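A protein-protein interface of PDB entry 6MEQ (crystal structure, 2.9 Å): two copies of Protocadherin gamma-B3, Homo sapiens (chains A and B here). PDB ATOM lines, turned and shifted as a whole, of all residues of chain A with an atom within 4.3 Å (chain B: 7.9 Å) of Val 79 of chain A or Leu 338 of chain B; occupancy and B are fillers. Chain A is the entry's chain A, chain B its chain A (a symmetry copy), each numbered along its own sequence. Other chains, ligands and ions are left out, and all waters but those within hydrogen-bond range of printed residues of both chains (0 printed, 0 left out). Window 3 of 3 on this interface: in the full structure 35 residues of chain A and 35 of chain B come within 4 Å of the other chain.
The backbone carbonyl oxygen (O) of Ser 321 of chain B sits at hydrogen-bond distance from the guanidinium group (NH2) of Arg 37 of chain A (3.0 Å).
The side-chain amino group (NZ) of Lys 340 of chain B lies within salt-bridge range of the side-chain carboxylate (OE2) of Glu 77 of chain A.
The backbone NH of Ile 39 of chain A is in hydrogen-bond range of the backbone carbonyl oxygen of Glu 77 of chain A (3.0 Å).
O of Ala 80 of chain A sits at hydrogen-bond distance from N of Asn 85 of chain A (3.2 Å).
N of Thr 318 of chain B lies within hydrogen-bond range of O of Lys 340 of chain B.
The backbone carbonyl oxygen (O) of Ala 320 of chain B sits at hydrogen-bond distance from the backbone NH (N) of Leu 338 of chain B, at 2.8 Å.
The backbone NH (N) of Val 336 of chain B is in hydrogen-bond range of the backbone carbonyl oxygen (O) of Leu 374 of chain B (2.9 Å).
The backbone NH of Tyr 372 of chain B lies within hydrogen-bond range of the backbone carbonyl oxygen of Ile 339 of chain B, at 2.8 Å.
CG2 of Thr 318 of chain B touches CG2 of Ile 39 of chain A (3.6 Å).
CG2 of Val 79 of chain A touches CB of Ala 320 of chain B, at 3.96 Å.
Val 79 of chain A touches Leu 338 of chain B.
Leu 84 of chain A touches Ala 335 of chain B (CD1 to O, 3.7 Å).
O of Val 336 of chain B touches CD1 of Leu 84 of chain A (3.2 Å).
Leu 84 of chain A touches Leu 338 of chain B.
CD1 of Leu 338 of chain B touches O of Asn 85 of chain A (3.4 Å).
Leu 338 of chain B touches Phe 86 of chain A (CB to CZ, 3.5 Å).
Ile 339 of chain B touches Phe 86 of chain A.
Phe 86 of chain A touches Thr 371 of chain B.
Of chain B, only Ala 320 and Leu 338 come within 4 Å of Val 79 of chain A.
Printed residues of chain A within 4 Å of Ser 321 of chain B: Arg 37 (3.0 Å).
Leu 338 of chain B touches four residues of chain A.
Asp 367 of chain B touches none of the printed residues of chain A.
Printed residues of chain A within 4 Å of Thr 371 of chain B: Phe 86.
Ile 408 of chain B touches none of the printed residues of chain A.
The nearest residue of chain B that does not touch Val 79 of chain A is Ser 321 of chain B (5.5 Å).
The nearest printed residue of chain B that does not touch Leu 84 of chain A is Ser 321 of chain B (4.02 Å).
Hydrophobic or aromatic side chains of chain B that line the printed part of chain A: Ala 320, Ala 335 and Leu 338.
Of the 11 printed residues of chain A, 7 touch a printed residue of chain B.
Among the printed residues, 12 pairs touch across the chains.
No position is printed for both chains.
Of the 12 pairs that touch across the chains among the printed residues, none has its exchanged pair printed and touching as well.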
ATOM      1  N   ASN A  35      29.961 -25.485  13.311  1.00  0.00           N
ATOM      2  CA  ASN A  35      30.166 -24.110  13.758  1.00  0.00           C
ATOM      3  C   ASN A  35      30.188 -24.015  15.279  1.00  0.00           C
ATOM      4  O   ASN A  35      29.213 -23.575  15.896  1.00  0.00           O
ATOM      5  CB  ASN A  35      29.084 -23.196  13.179  1.00  0.00           C
ATOM      6  CG  ASN A  35      29.335 -21.729  13.480  1.00  0.00           C
ATOM      7  OD1 ASN A  35      30.469 -21.321  13.735  1.00  0.00           O
ATOM      8  ND2 ASN A  35      28.276 -20.930  13.452  1.00  0.00           N
ATOM      9  N   LEU A  36      31.295 -24.428  15.891  1.00  0.00           N
ATOM     10  CA  LEU A  36      31.384 -24.440  17.344  1.00  0.00           C
ATOM     11  C   LEU A  36      31.523 -23.025  17.891  1.00  0.00           C
ATOM     12  O   LEU A  36      32.166 -22.163  17.284  1.00  0.00           O
ATOM     13  CB  LEU A  36      32.567 -25.294  17.793  1.00  0.00           C
ATOM     14  CG  LEU A  36      32.500 -26.774  17.412  1.00  0.00           C
ATOM     15  CD1 LEU A  36      33.690 -27.533  17.976  1.00  0.00           C
ATOM     16  CD2 LEU A  36      31.196 -27.380  17.894  1.00  0.00           C
ATOM     17  N   ARG A  37      30.910 -22.790  19.049  1.00  0.00           N
ATOM     18  CA  ARG A  37      30.991 -21.500  19.717  1.00  0.00           C
ATOM     19  C   ARG A  37      30.737 -21.703  21.202  1.00  0.00           C
ATOM     20  O   ARG A  37      29.990 -22.601  21.601  1.00  0.00           O
ATOM     21  CB  ARG A  37      29.991 -20.497  19.131  1.00  0.00           C
ATOM     22  CG  ARG A  37      28.538 -20.931  19.227  1.00  0.00           C
ATOM     23  CD  ARG A  37      27.613 -19.898  18.606  1.00  0.00           C
ATOM     24  NE  ARG A  37      26.209 -20.289  18.701  1.00  0.00           N
ATOM     25  CZ  ARG A  37      25.576 -21.030  17.797  1.00  0.00           C
ATOM     26  NH1 ARG A  37      26.223 -21.467  16.725  1.00  0.00           N
ATOM     27  NH2 ARG A  37      24.297 -21.336  17.966  1.00  0.00           N
ATOM     28  N   ILE A  39      29.345 -20.343  24.878  1.00  0.00           N
ATOM     29  CA  ILE A  39      28.250 -19.532  25.396  1.00  0.00           C
ATOM     30  C   ILE A  39      28.472 -19.354  26.892  1.00  0.00           C
ATOM     31  O   ILE A  39      28.264 -20.292  27.674  1.00  0.00           O
ATOM     32  CB  ILE A  39      26.880 -20.160  25.111  1.00  0.00           C
ATOM     33  CG1 ILE A  39      26.640 -20.249  23.604  1.00  0.00           C
ATOM     34  CG2 ILE A  39      25.779 -19.352  25.774  1.00  0.00           C
ATOM     35  CD1 ILE A  39      26.629 -18.907  22.905  1.00  0.00           C
ATOM     36  N   GLU A  77      28.905 -23.854  28.445  1.00  0.00           N
ATOM     37  CA  GLU A  77      28.258 -24.732  27.479  1.00  0.00           C
ATOM     38  C   GLU A  77      28.695 -24.349  26.074  1.00  0.00           C
ATOM     39  O   GLU A  77      28.613 -23.178  25.691  1.00  0.00           O
ATOM     40  CB  GLU A  77      26.730 -24.651  27.594  1.00  0.00           C
ATOM     41  CG  GLU A  77      26.178 -25.097  28.938  1.00  0.00           C
ATOM     42  CD  GLU A  77      26.228 -26.601  29.123  1.00  0.00           C
ATOM     43  OE1 GLU A  77      26.365 -27.322  28.114  1.00  0.00           O
ATOM     44  OE2 GLU A  77      26.129 -27.062  30.281  1.00  0.00           O
ATOM     45  N   MET A  78      29.158 -25.336  25.312  1.00  0.00           N
ATOM     46  CA  MET A  78      29.497 -25.151  23.910  1.00  0.00           C
ATOM     47  C   MET A  78      28.322 -25.587  23.045  1.00  0.00           C
ATOM     48  O   MET A  78      27.703 -26.625  23.298  1.00  0.00           O
ATOM     49  CB  MET A  78      30.748 -25.946  23.534  1.00  0.00           C
ATOM     50  CG  MET A  78      31.269 -25.648  22.137  1.00  0.00           C
ATOM     51  SD  MET A  78      32.545 -26.801  21.600  1.00  0.00           S
ATOM     52  CE  MET A  78      31.604 -28.322  21.510  1.00  0.00           C
ATOM     53  N   VAL A  79      28.019 -24.791  22.024  1.00  0.00           N
ATOM     54  CA  VAL A  79      26.858 -25.007  21.168  1.00  0.00           C
ATOM     55  C   VAL A  79      27.332 -25.432  19.787  1.00  0.00           C
ATOM     56  O   VAL A  79      28.167 -24.756  19.172  1.00  0.00           O
ATOM     57  CB  VAL A  79      25.979 -23.747  21.082  1.00  0.00           C
ATOM     58  CG1 VAL A  79      24.875 -23.940  20.055  1.00  0.00           C
ATOM     59  CG2 VAL A  79      25.391 -23.423  22.444  1.00  0.00           C
ATOM     60  N   ALA A  80      26.800 -26.551  19.304  1.00  0.00           N
ATOM     61  CA  ALA A  80      27.015 -27.021  17.944  1.00  0.00           C
ATOM     62  C   ALA A  80      25.674 -27.084  17.229  1.00  0.00           C
ATOM     63  O   ALA A  80      24.658 -27.434  17.837  1.00  0.00           O
ATOM     64  CB  ALA A  80      27.687 -28.397  17.927  1.00  0.00           C
ATOM     65  N   LEU A  84      21.445 -29.368  16.597  1.00  0.00           N
ATOM     66  CA  LEU A  84      21.696 -28.550  17.776  1.00  0.00           C
ATOM     67  C   LEU A  84      21.830 -29.445  19.003  1.00  0.00           C
ATOM     68  O   LEU A  84      20.925 -30.228  19.309  1.00  0.00           O
ATOM     69  CB  LEU A  84      20.578 -27.529  17.975  1.00  0.00           C
ATOM     70  CG  LEU A  84      20.694 -26.248  17.148  1.00  0.00           C
ATOM     71  CD1 LEU A  84      19.454 -25.396  17.318  1.00  0.00           C
ATOM     72  CD2 LEU A  84      21.934 -25.468  17.553  1.00  0.00           C
ATOM     73  N   ASN A  85      22.957 -29.322  19.702  1.00  0.00           N
ATOM     74  CA  ASN A  85      23.211 -30.099  20.906  1.00  0.00           C
ATOM     75  C   ASN A  85      24.013 -29.256  21.885  1.00  0.00           C
ATOM     76  O   ASN A  85      24.655 -28.270  21.510  1.00  0.00           O
ATOM     77  CB  ASN A  85      23.956 -31.404  20.595  1.00  0.00           C
ATOM     78  CG  ASN A  85      23.061 -32.454  19.968  1.00  0.00           C
ATOM     79  OD1 ASN A  85      21.916 -32.640  20.383  1.00  0.00           O
ATOM     80  ND2 ASN A  85      23.579 -33.148  18.962  1.00  0.00           N
ATOM     81  N   PHE A  86      23.967 -29.657  23.150  1.00  0.00           N
ATOM     82  CA  PHE A  86      24.727 -29.016  24.212  1.00  0.00           C
ATOM     83  C   PHE A  86      25.918 -29.882  24.603  1.00  0.00           C
ATOM     84  O   PHE A  86      25.851 -31.114  24.578  1.00  0.00           O
ATOM     85  CB  PHE A  86      23.849 -28.757  25.437  1.00  0.00           C
ATOM     86  CG  PHE A  86      23.303 -27.358  25.509  1.00  0.00           C
ATOM     87  CD1 PHE A  86      24.003 -26.297  24.959  1.00  0.00           C
ATOM     88  CD2 PHE A  86      22.092 -27.105  26.131  1.00  0.00           C
ATOM     89  CE1 PHE A  86      23.504 -25.010  25.027  1.00  0.00           C
ATOM     90  CE2 PHE A  86      21.587 -25.820  26.202  1.00  0.00           C
ATOM     91  CZ  PHE A  86      22.295 -24.771  25.650  1.00  0.00           C
ATOM     92  N   ILE B 317      17.881 -17.094  31.818  1.00  0.00           N
ATOM     93  CA  ILE B 317      17.577 -17.885  30.632  1.00  0.00           C
ATOM     94  C   ILE B 317      18.602 -17.560  29.556  1.00  0.00           C
ATOM     95  O   ILE B 317      18.876 -16.384  29.286  1.00  0.00           O
ATOM     96  CB  ILE B 317      16.148 -17.617  30.123  1.00  0.00           C
ATOM     97  CG1 ILE B 317      15.123 -17.960  31.206  1.00  0.00           C
ATOM     98  CG2 ILE B 317      15.874 -18.409  28.855  1.00  0.00           C
ATOM     99  CD1 ILE B 317      13.690 -17.703  30.792  1.00  0.00           C
ATOM    100  N   THR B 318      19.166 -18.600  28.944  1.00  0.00           N
ATOM    101  CA  THR B 318      20.126 -18.455  27.860  1.00  0.00           C
ATOM    102  C   THR B 318      19.636 -19.255  26.663  1.00  0.00           C
ATOM    103  O   THR B 318      19.215 -20.407  26.816  1.00  0.00           O
ATOM    104  CB  THR B 318      21.521 -18.929  28.281  1.00  0.00           C
ATOM    105  OG1 THR B 318      21.914 -18.254  29.482  1.00  0.00           O
ATOM    106  CG2 THR B 318      22.533 -18.632  27.190  1.00  0.00           C
ATOM    107  N   LEU B 319      19.690 -18.649  25.481  1.00  0.00           N
ATOM    108  CA  LEU B 319      19.170 -19.258  24.267  1.00  0.00           C
ATOM    109  C   LEU B 319      20.248 -19.315  23.192  1.00  0.00           C
ATOM    110  O   LEU B 319      21.203 -18.533  23.192  1.00  0.00           O
ATOM    111  CB  LEU B 319      17.950 -18.489  23.743  1.00  0.00           C
ATOM    112  CG  LEU B 319      16.770 -18.381  24.711  1.00  0.00           C
ATOM    113  CD1 LEU B 319      15.663 -17.527  24.118  1.00  0.00           C
ATOM    114  CD2 LEU B 319      16.248 -19.764  25.075  1.00  0.00           C
ATOM    115  N   ALA B 320      20.076 -20.261  22.270  1.00  0.00           N
ATOM    116  CA  ALA B 320      20.983 -20.430  21.144  1.00  0.00           C
ATOM    117  C   ALA B 320      20.252 -21.190  20.048  1.00  0.00           C
ATOM    118  O   ALA B 320      19.486 -22.115  20.334  1.00  0.00           O
ATOM    119  CB  ALA B 320      22.259 -21.175  21.553  1.00  0.00           C
ATOM    120  N   SER B 321      20.489 -20.797  18.799  1.00  0.00           N
ATOM    121  CA  SER B 321      19.812 -21.407  17.663  1.00  0.00           C
ATOM    122  C   SER B 321      20.682 -21.255  16.423  1.00  0.00           C
ATOM    123  O   SER B 321      21.781 -20.694  16.472  1.00  0.00           O
ATOM    124  CB  SER B 321      18.429 -20.783  17.449  1.00  0.00           C
ATOM    125  OG  SER B 321      18.532 -19.395  17.185  1.00  0.00           O
ATOM    126  N   GLU B 322      20.175 -21.765  15.300  1.00  0.00           N
ATOM    127  CA  GLU B 322      20.867 -21.671  14.013  1.00  0.00           C
ATOM    128  C   GLU B 322      20.511 -20.340  13.349  1.00  0.00           C
ATOM    129  O   GLU B 322      19.759 -20.262  12.374  1.00  0.00           O
ATOM    130  CB  GLU B 322      20.509 -22.860  13.130  1.00  0.00           C
ATOM    131  CG  GLU B 322      21.249 -22.915  11.800  1.00  0.00           C
ATOM    132  CD  GLU B 322      20.787 -24.061  10.922  1.00  0.00           C
ATOM    133  OE1 GLU B 322      20.155 -25.000  11.450  1.00  0.00           O
ATOM    134  OE2 GLU B 322      21.050 -24.020   9.702  1.00  0.00           O
ATOM    135  N   ALA B 335      15.658 -30.205  16.563  1.00  0.00           N
ATOM    136  CA  ALA B 335      15.983 -29.193  17.557  1.00  0.00           C
ATOM    137  C   ALA B 335      16.097 -27.826  16.893  1.00  0.00           C
ATOM    138  O   ALA B 335      16.840 -27.655  15.921  1.00  0.00           O
ATOM    139  CB  ALA B 335      17.285 -29.546  18.274  1.00  0.00           C
ATOM    140  N   VAL B 336      15.359 -26.852  17.420  1.00  0.00           N
ATOM    141  CA  VAL B 336      15.327 -25.507  16.870  1.00  0.00           C
ATOM    142  C   VAL B 336      16.073 -24.517  17.757  1.00  0.00           C
ATOM    143  O   VAL B 336      16.800 -23.657  17.254  1.00  0.00           O
ATOM    144  CB  VAL B 336      13.871 -25.050  16.636  1.00  0.00           C
ATOM    145  CG1 VAL B 336      13.811 -23.554  16.395  1.00  0.00           C
ATOM    146  CG2 VAL B 336      13.271 -25.800  15.461  1.00  0.00           C
ATOM    147  N   ALA B 337      15.915 -24.626  19.073  1.00  0.00           N
ATOM    148  CA  ALA B 337      16.584 -23.736  20.006  1.00  0.00           C
ATOM    149  C   ALA B 337      17.049 -24.527  21.218  1.00  0.00           C
ATOM    150  O   ALA B 337      16.466 -25.557  21.569  1.00  0.00           O
ATOM    151  CB  ALA B 337      15.669 -22.586  20.448  1.00  0.00           C
ATOM    152  N   LEU B 338      18.110 -24.037  21.851  1.00  0.00           N
ATOM    153  CA  LEU B 338      18.663 -24.634  23.059  1.00  0.00           C
ATOM    154  C   LEU B 338      18.444 -23.683  24.227  1.00  0.00           C
ATOM    155  O   LEU B 338      18.722 -22.484  24.115  1.00  0.00           O
ATOM    156  CB  LEU B 338      20.153 -24.937  22.889  1.00  0.00           C
ATOM    157  CG  LEU B 338      20.536 -25.840  21.715  1.00  0.00           C
ATOM    158  CD1 LEU B 338      22.039 -26.068  21.681  1.00  0.00           C
ATOM    159  CD2 LEU B 338      19.791 -27.162  21.791  1.00  0.00           C
ATOM    160  N   ILE B 339      17.947 -24.216  25.340  1.00  0.00           N
ATOM    161  CA  ILE B 339      17.618 -23.427  26.522  1.00  0.00           C
ATOM    162  C   ILE B 339      18.548 -23.832  27.655  1.00  0.00           C
ATOM    163  O   ILE B 339      18.683 -25.023  27.963  1.00  0.00           O
ATOM    164  CB  ILE B 339      16.145 -23.609  26.929  1.00  0.00           C
ATOM    165  CG1 ILE B 339      15.222 -23.289  25.751  1.00  0.00           C
ATOM    166  CG2 ILE B 339      15.810 -22.732  28.125  1.00  0.00           C
ATOM    167  CD1 ILE B 339      13.751 -23.466  26.063  1.00  0.00           C
ATOM    168  N   LYS B 340      19.187 -22.841  28.276  1.00  0.00           N
ATOM    169  CA  LYS B 340      20.074 -23.055  29.412  1.00  0.00           C
ATOM    170  C   LYS B 340      19.632 -22.158  30.557  1.00  0.00           C
ATOM    171  O   LYS B 340      19.472 -20.947  30.374  1.00  0.00           O
ATOM    172  CB  LYS B 340      21.532 -22.767  29.042  1.00  0.00           C
ATOM    173  CG  LYS B 340      22.494 -22.807  30.219  1.00  0.00           C
ATOM    174  CD  LYS B 340      22.532 -24.184  30.861  1.00  0.00           C
ATOM    175  CE  LYS B 340      23.442 -24.201  32.080  1.00  0.00           C
ATOM    176  NZ  LYS B 340      24.839 -23.811  31.741  1.00  0.00           N
ATOM    177  N   THR B 341      19.434 -22.751  31.733  1.00  0.00           N
ATOM    178  CA  THR B 341      18.978 -22.026  32.908  1.00  0.00           C
ATOM    179  C   THR B 341      19.903 -22.310  34.083  1.00  0.00           C
ATOM    180  O   THR B 341      20.540 -23.364  34.152  1.00  0.00           O
ATOM    181  CB  THR B 341      17.538 -22.407  33.291  1.00  0.00           C
ATOM    182  OG1 THR B 341      17.473 -23.809  33.585  1.00  0.00           O
ATOM    183  CG2 THR B 341      16.574 -22.087  32.156  1.00  0.00           C
ATOM    184  N   ASP B 367      16.396 -32.224  28.857  1.00  0.00           N
ATOM    185  CA  ASP B 367      17.489 -33.184  28.763  1.00  0.00           C
ATOM    186  C   ASP B 367      18.082 -33.452  30.140  1.00  0.00           C
ATOM    187  O   ASP B 367      17.915 -34.544  30.694  1.00  0.00           O
ATOM    188  CB  ASP B 367      18.570 -32.679  27.806  1.00  0.00           C
ATOM    189  CG  ASP B 367      18.044 -32.451  26.403  1.00  0.00           C
ATOM    190  OD1 ASP B 367      17.052 -33.108  26.023  1.00  0.00           O
ATOM    191  OD2 ASP B 367      18.625 -31.616  25.679  1.00  0.00           O
ATOM    192  N   ASN B 370      19.335 -28.569  33.781  1.00  0.00           N
ATOM    193  CA  ASN B 370      19.376 -27.169  33.376  1.00  0.00           C
ATOM    194  C   ASN B 370      19.468 -26.976  31.866  1.00  0.00           C
ATOM    195  O   ASN B 370      19.774 -25.865  31.418  1.00  0.00           O
ATOM    196  CB  ASN B 370      20.554 -26.460  34.056  1.00  0.00           C
ATOM    197  CG  ASN B 370      20.362 -26.316  35.553  1.00  0.00           C
ATOM    198  OD1 ASN B 370      19.235 -26.226  36.041  1.00  0.00           O
ATOM    199  ND2 ASN B 370      21.466 -26.292  36.292  1.00  0.00           N
ATOM    200  N   THR B 371      19.210 -28.011  31.070  1.00  0.00           N
ATOM    201  CA  THR B 371      19.295 -27.915  29.619  1.00  0.00           C
ATOM    202  C   THR B 371      17.977 -28.358  29.001  1.00  0.00           C
ATOM    203  O   THR B 371      17.420 -29.389  29.389  1.00  0.00           O
ATOM    204  CB  THR B 371      20.444 -28.765  29.066  1.00  0.00           C
ATOM    205  OG1 THR B 371      20.261 -30.132  29.454  1.00  0.00           O
ATOM    206  CG2 THR B 371      21.782 -28.265  29.597  1.00  0.00           C
ATOM    207  N   TYR B 372      17.485 -27.577  28.041  1.00  0.00           N
ATOM    208  CA  TYR B 372      16.248 -27.875  27.336  1.00  0.00           C
ATOM    209  C   TYR B 372      16.462 -27.684  25.840  1.00  0.00           C
ATOM    210  O   TYR B 372      17.422 -27.044  25.404  1.00  0.00           O
ATOM    211  CB  TYR B 372      15.091 -26.986  27.815  1.00  0.00           C
ATOM    212  CG  TYR B 372      14.793 -27.093  29.294  1.00  0.00           C
ATOM    213  CD1 TYR B 372      13.805 -27.948  29.763  1.00  0.00           C
ATOM    214  CD2 TYR B 372      15.494 -26.332  30.222  1.00  0.00           C
ATOM    215  CE1 TYR B 372      13.526 -28.047  31.115  1.00  0.00           C
ATOM    216  CE2 TYR B 372      15.224 -26.424  31.574  1.00  0.00           C
ATOM    217  CZ  TYR B 372      14.239 -27.283  32.015  1.00  0.00           C
ATOM    218  OH  TYR B 372      13.965 -27.379  33.360  1.00  0.00           O
ATOM    219  N   ARG B 373      15.548 -28.251  25.053  1.00  0.00           N
ATOM    220  CA  ARG B 373      15.593 -28.135  23.602  1.00  0.00           C
ATOM    221  C   ARG B 373      14.202 -27.823  23.078  1.00  0.00           C
ATOM    222  O   ARG B 373      13.239 -28.519  23.416  1.00  0.00           O
ATOM    223  CB  ARG B 373      16.124 -29.421  22.953  1.00  0.00           C
ATOM    224  CG  ARG B 373      17.583 -29.717  23.259  1.00  0.00           C
ATOM    225  CD  ARG B 373      18.093 -30.930  22.489  1.00  0.00           C
ATOM    226  NE  ARG B 373      17.410 -32.163  22.872  1.00  0.00           N
ATOM    227  CZ  ARG B 373      16.455 -32.745  22.152  1.00  0.00           C
ATOM    228  NH1 ARG B 373      16.068 -32.209  21.003  1.00  0.00           N
ATOM    229  NH2 ARG B 373      15.890 -33.865  22.581  1.00  0.00           N
ATOM    230  N   LEU B 374      14.099 -26.780  22.258  1.00  0.00           N
ATOM    231  CA  LEU B 374      12.832 -26.405  21.633  1.00  0.00           C
ATOM    232  C   LEU B 374      12.637 -27.274  20.397  1.00  0.00           C
ATOM    233  O   LEU B 374      13.267 -27.055  19.360  1.00  0.00           O
ATOM    234  CB  LEU B 374      12.824 -24.922  21.283  1.00  0.00           C
ATOM    235  CG  LEU B 374      11.472 -24.334  20.873  1.00  0.00           C
ATOM    236  CD1 LEU B 374      10.466 -24.482  22.002  1.00  0.00           C
ATOM    237  CD2 LEU B 374      11.618 -22.875  20.468  1.00  0.00           C
ATOM    238  N   VAL B 375      11.757 -28.266  20.506  1.00  0.00           N
ATOM    239  CA  VAL B 375      11.533 -29.260  19.462  1.00  0.00           C
ATOM    240  C   VAL B 375      10.216 -28.958  18.759  1.00  0.00           C
ATOM    241  O   VAL B 375       9.210 -28.644  19.409  1.00  0.00           O
ATOM    242  CB  VAL B 375      11.537 -30.681  20.057  1.00  0.00           C
ATOM    243  CG1 VAL B 375      11.206 -31.710  18.998  1.00  0.00           C
ATOM    244  CG2 VAL B 375      12.886 -30.986  20.698  1.00  0.00           C
ATOM    245  N   ILE B 392       9.960 -17.893  26.414  1.00  0.00           N
ATOM    246  CA  ILE B 392      10.318 -18.895  27.411  1.00  0.00           C
ATOM    247  C   ILE B 392      10.291 -18.237  28.784  1.00  0.00           C
ATOM    248  O   ILE B 392      10.864 -17.156  28.971  1.00  0.00           O
ATOM    249  CB  ILE B 392      11.698 -19.508  27.122  1.00  0.00           C
ATOM    250  CG1 ILE B 392      11.732 -20.109  25.716  1.00  0.00           C
ATOM    251  CG2 ILE B 392      12.044 -20.562  28.164  1.00  0.00           C
ATOM    252  CD1 ILE B 392      10.714 -21.208  25.498  1.00  0.00           C
ATOM    253  N   ILE B 408      12.336 -14.946  21.930  1.00  0.00           N
ATOM    254  CA  ILE B 408      13.231 -15.089  20.789  1.00  0.00           C
ATOM    255  C   ILE B 408      12.387 -15.219  19.527  1.00  0.00           C
ATOM    256  O   ILE B 408      11.349 -15.890  19.528  1.00  0.00           O
ATOM    257  CB  ILE B 408      14.177 -16.298  20.953  1.00  0.00           C
ATOM    258  CG1 ILE B 408      15.104 -16.434  19.742  1.00  0.00           C
ATOM    259  CG2 ILE B 408      13.387 -17.581  21.182  1.00  0.00           C
ATOM    260  CD1 ILE B 408      16.060 -17.603  19.833  1.00  0.00           C
